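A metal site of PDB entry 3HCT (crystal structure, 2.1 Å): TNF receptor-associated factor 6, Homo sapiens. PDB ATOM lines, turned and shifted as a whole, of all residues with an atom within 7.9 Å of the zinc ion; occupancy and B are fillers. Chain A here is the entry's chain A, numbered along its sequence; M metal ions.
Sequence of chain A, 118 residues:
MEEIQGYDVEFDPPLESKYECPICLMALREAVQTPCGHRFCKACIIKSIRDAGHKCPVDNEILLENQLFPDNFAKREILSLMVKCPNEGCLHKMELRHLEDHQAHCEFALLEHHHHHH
The backbone carbonyl oxygen (O) of Glu 61 lies within hydrogen-bond range of the backbone NH (N) of Cys 56 (2.7 Å). The backbone NH of Glu 61 sits close to the side-chain carboxylate of Asp 59, 3.2 Å away. The side-chain hydroxyl of Thr 34 lies close to the backbone NH of Cys 36. SG of Cys 56 lies close to N of Val 58. N of His 38 lies within hydrogen-bond range of OG1 of Thr 34 (3.1 Å).
Merely in contact with the zinc ion: Thr 34 (3.9 Å). The nearest printed residue that does not touch the zinc ion is Val 58 (4.5 Å).
The zinc ion is bound by ND1 of His 38, 2.1 Å away. The zinc ion is bound by SG of Cys 56. The zinc ion is bound by SG of Cys 36. The side-chain carboxylate (OD1) of Asp 59 is bound to the zinc ion (2.6 Å). Slightly farther from the zinc ion lies the side-chain carboxylate (OD2) of Asp 59 (2.6 Å).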
ATOM      1  N   THR A  34      -0.167 -33.175  19.849  1.00  0.00           N
ATOM      2  CA  THR A  34      -1.046 -33.403  20.964  1.00  0.00           C
ATOM      3  C   THR A  34      -2.474 -32.982  20.632  1.00  0.00           C
ATOM      4  O   THR A  34      -2.711 -32.296  19.638  1.00  0.00           O
ATOM      5  CB  THR A  34      -0.582 -32.619  22.209  1.00  0.00           C
ATOM      6  OG1 THR A  34      -0.641 -31.209  21.936  1.00  0.00           O
ATOM      7  CG2 THR A  34       0.860 -33.003  22.570  1.00  0.00           C
ATOM      8  N   PRO A  35      -3.447 -33.417  21.440  1.00  0.00           N
ATOM      9  CA  PRO A  35      -4.840 -33.041  21.183  1.00  0.00           C
ATOM     10  C   PRO A  35      -4.980 -31.507  21.211  1.00  0.00           C
ATOM     11  O   PRO A  35      -5.854 -30.945  20.546  1.00  0.00           O
ATOM     12  CB  PRO A  35      -5.588 -33.717  22.322  1.00  0.00           C
ATOM     13  CG  PRO A  35      -4.774 -34.969  22.554  1.00  0.00           C
ATOM     14  CD  PRO A  35      -3.357 -34.435  22.507  1.00  0.00           C
ATOM     15  N   CYS A  36      -4.113 -30.848  21.968  1.00  0.00           N
ATOM     16  CA  CYS A  36      -4.147 -29.388  22.062  1.00  0.00           C
ATOM     17  C   CYS A  36      -3.417 -28.686  20.912  1.00  0.00           C
ATOM     18  O   CYS A  36      -3.214 -27.465  20.963  1.00  0.00           O
ATOM     19  CB  CYS A  36      -3.589 -28.916  23.410  1.00  0.00           C
ATOM     20  SG  CYS A  36      -2.107 -29.785  23.954  1.00  0.00           S
ATOM     21  N   GLY A  37      -3.037 -29.450  19.895  1.00  0.00           N
ATOM     22  CA  GLY A  37      -2.383 -28.889  18.726  1.00  0.00           C
ATOM     23  C   GLY A  37      -0.886 -28.634  18.744  1.00  0.00           C
ATOM     24  O   GLY A  37      -0.366 -27.995  17.821  1.00  0.00           O
ATOM     25  N   HIS A  38      -0.171 -29.100  19.761  1.00  0.00           N
ATOM     26  CA  HIS A  38       1.264 -28.852  19.796  1.00  0.00           C
ATOM     27  C   HIS A  38       2.120 -30.018  19.318  1.00  0.00           C
ATOM     28  O   HIS A  38       1.740 -31.182  19.469  1.00  0.00           O
ATOM     29  CB  HIS A  38       1.664 -28.372  21.206  1.00  0.00           C
ATOM     30  CG  HIS A  38       1.096 -27.037  21.542  1.00  0.00           C
ATOM     31  ND1 HIS A  38      -0.006 -26.887  22.354  1.00  0.00           N
ATOM     32  CD2 HIS A  38       1.384 -25.798  21.073  1.00  0.00           C
ATOM     33  CE1 HIS A  38      -0.381 -25.618  22.361  1.00  0.00           C
ATOM     34  NE2 HIS A  38       0.455 -24.930  21.596  1.00  0.00           N
ATOM     35  N   ARG A  39       3.261 -29.697  18.717  1.00  0.00           N
ATOM     36  CA  ARG A  39       4.170 -30.692  18.159  1.00  0.00           C
ATOM     37  C   ARG A  39       5.509 -30.828  18.885  1.00  0.00           C
ATOM     38  O   ARG A  39       6.080 -29.850  19.375  1.00  0.00           O
ATOM     39  CB  ARG A  39       4.461 -30.372  16.682  1.00  0.00           C
ATOM     40  CG  ARG A  39       3.229 -30.294  15.794  1.00  0.00           C
ATOM     41  CD  ARG A  39       3.613 -30.040  14.329  1.00  0.00           C
ATOM     42  NE  ARG A  39       2.422 -29.913  13.478  1.00  0.00           N
ATOM     43  CZ  ARG A  39       1.608 -28.858  13.479  1.00  0.00           C
ATOM     44  NH1 ARG A  39       1.854 -27.826  14.277  1.00  0.00           N
ATOM     45  NH2 ARG A  39       0.534 -28.849  12.690  1.00  0.00           N
ATOM     46  N   PHE A  40       6.021 -32.052  18.910  1.00  0.00           N
ATOM     47  CA  PHE A  40       7.283 -32.365  19.560  1.00  0.00           C
ATOM     48  C   PHE A  40       7.939 -33.591  18.913  1.00  0.00           C
ATOM     49  O   PHE A  40       7.323 -34.298  18.121  1.00  0.00           O
ATOM     50  CB  PHE A  40       7.077 -32.715  21.045  1.00  0.00           C
ATOM     51  CG  PHE A  40       6.311 -31.693  21.826  1.00  0.00           C
ATOM     52  CD1 PHE A  40       4.913 -31.735  21.876  1.00  0.00           C
ATOM     53  CD2 PHE A  40       6.975 -30.679  22.525  1.00  0.00           C
ATOM     54  CE1 PHE A  40       4.201 -30.795  22.613  1.00  0.00           C
ATOM     55  CE2 PHE A  40       6.263 -29.739  23.262  1.00  0.00           C
ATOM     56  CZ  PHE A  40       4.869 -29.805  23.306  1.00  0.00           C
ATOM     57  N   LYS A  55       1.607 -33.202  31.205  1.00  0.00           N
ATOM     58  CA  LYS A  55       1.032 -31.955  30.709  1.00  0.00           C
ATOM     59  C   LYS A  55       1.756 -31.497  29.462  1.00  0.00           C
ATOM     60  O   LYS A  55       2.924 -31.812  29.258  1.00  0.00           O
ATOM     61  CB  LYS A  55       1.165 -30.854  31.769  1.00  0.00           C
ATOM     62  CG  LYS A  55       0.193 -30.968  32.924  1.00  0.00           C
ATOM     63  CD  LYS A  55       0.355 -29.785  33.872  1.00  0.00           C
ATOM     64  CE  LYS A  55      -0.762 -29.771  34.895  1.00  0.00           C
ATOM     65  NZ  LYS A  55      -0.894 -31.081  35.575  1.00  0.00           N
ATOM     66  N   CYS A  56       1.052 -30.748  28.608  1.00  0.00           N
ATOM     67  CA  CYS A  56       1.686 -30.216  27.411  1.00  0.00           C
ATOM     68  C   CYS A  56       2.508 -29.042  27.934  1.00  0.00           C
ATOM     69  O   CYS A  56       1.959 -28.093  28.502  1.00  0.00           O
ATOM     70  CB  CYS A  56       0.650 -29.687  26.420  1.00  0.00           C
ATOM     71  SG  CYS A  56       1.461 -28.840  25.075  1.00  0.00           S
ATOM     72  N   PRO A  57       3.839 -29.075  27.743  1.00  0.00           N
ATOM     73  CA  PRO A  57       4.663 -27.966  28.239  1.00  0.00           C
ATOM     74  C   PRO A  57       4.341 -26.581  27.690  1.00  0.00           C
ATOM     75  O   PRO A  57       4.618 -25.584  28.340  1.00  0.00           O
ATOM     76  CB  PRO A  57       6.081 -28.430  27.918  1.00  0.00           C
ATOM     77  CG  PRO A  57       5.903 -29.306  26.714  1.00  0.00           C
ATOM     78  CD  PRO A  57       4.660 -30.098  27.062  1.00  0.00           C
ATOM     79  N   VAL A  58       3.723 -26.502  26.506  1.00  0.00           N
ATOM     80  CA  VAL A  58       3.395 -25.200  25.916  1.00  0.00           C
ATOM     81  C   VAL A  58       2.213 -24.511  26.591  1.00  0.00           C
ATOM     82  O   VAL A  58       2.285 -23.341  26.932  1.00  0.00           O
ATOM     83  CB  VAL A  58       3.096 -25.332  24.391  1.00  0.00           C
ATOM     84  CG1 VAL A  58       2.653 -23.975  23.811  1.00  0.00           C
ATOM     85  CG2 VAL A  58       4.352 -25.819  23.663  1.00  0.00           C
ATOM     86  N   ASP A  59       1.111 -25.235  26.806  1.00  0.00           N
ATOM     87  CA  ASP A  59      -0.055 -24.620  27.417  1.00  0.00           C
ATOM     88  C   ASP A  59      -0.513 -25.220  28.740  1.00  0.00           C
ATOM     89  O   ASP A  59      -1.524 -24.785  29.303  1.00  0.00           O
ATOM     90  CB  ASP A  59      -1.222 -24.619  26.413  1.00  0.00           C
ATOM     91  CG  ASP A  59      -1.462 -25.991  25.828  1.00  0.00           C
ATOM     92  OD1 ASP A  59      -1.005 -26.976  26.434  1.00  0.00           O
ATOM     93  OD2 ASP A  59      -2.127 -26.086  24.778  1.00  0.00           O
ATOM     94  N   ASN A  60       0.227 -26.200  29.251  1.00  0.00           N
ATOM     95  CA  ASN A  60      -0.119 -26.839  30.516  1.00  0.00           C
ATOM     96  C   ASN A  60      -1.398 -27.677  30.489  1.00  0.00           C
ATOM     97  O   ASN A  60      -1.984 -27.951  31.541  1.00  0.00           O
ATOM     98  CB  ASN A  60      -0.237 -25.808  31.642  1.00  0.00           C
ATOM     99  CG  ASN A  60       1.092 -25.203  32.035  1.00  0.00           C
ATOM    100  OD1 ASN A  60       2.072 -25.919  32.275  1.00  0.00           O
ATOM    101  ND2 ASN A  60       1.137 -23.876  32.133  1.00  0.00           N
ATOM    102  N   GLU A  61      -1.857 -28.073  29.304  1.00  0.00           N
ATOM    103  CA  GLU A  61      -3.053 -28.905  29.197  1.00  0.00           C
ATOM    104  C   GLU A  61      -2.674 -30.309  29.660  1.00  0.00           C
ATOM    105  O   GLU A  61      -1.538 -30.740  29.468  1.00  0.00           O
ATOM    106  CB  GLU A  61      -3.538 -28.986  27.734  1.00  0.00           C
ATOM    107  CG  GLU A  61      -4.060 -27.688  27.136  1.00  0.00           C
ATOM    108  CD  GLU A  61      -5.471 -27.345  27.587  1.00  0.00           C
ATOM    109  OE1 GLU A  61      -6.270 -28.280  27.803  1.00  0.00           O
ATOM    110  OE2 GLU A  61      -5.798 -26.141  27.704  1.00  0.00           O
ATOM    111  N   ILE A  62      -3.610 -31.019  30.272  1.00  0.00           N
ATOM    112  CA  ILE A  62      -3.337 -32.384  30.712  1.00  0.00           C
ATOM    113  C   ILE A  62      -2.933 -33.168  29.468  1.00  0.00           C
ATOM    114  O   ILE A  62      -3.568 -33.055  28.426  1.00  0.00           O
ATOM    115  CB  ILE A  62      -4.588 -33.061  31.311  1.00  0.00           C
ATOM    116  CG1 ILE A  62      -4.315 -34.563  31.499  1.00  0.00           C
ATOM    117  CG2 ILE A  62      -5.783 -32.807  30.416  1.00  0.00           C
ATOM    118  CD1 ILE A  62      -5.548 -35.389  31.740  1.00  0.00           C
ATOM    119  N   LEU A  63      -1.875 -33.976  29.589  1.00  0.00           N
ATOM    120  CA  LEU A  63      -1.407 -34.738  28.447  1.00  0.00           C
ATOM    121  C   LEU A  63      -1.017 -36.141  28.860  1.00  0.00           C
ATOM    122  O   LEU A  63      -0.210 -36.326  29.785  1.00  0.00           O
ATOM    123  CB  LEU A  63      -0.201 -34.044  27.807  1.00  0.00           C
ATOM    124  CG  LEU A  63       0.370 -34.634  26.519  1.00  0.00           C
ATOM    125  CD1 LEU A  63      -0.751 -34.765  25.475  1.00  0.00           C
ATOM    126  CD2 LEU A  63       1.494 -33.754  25.995  1.00  0.00           C
HETATM  127 ZN    ZN M   1      -0.497 -28.004  24.121  1.00  0.00          ZN
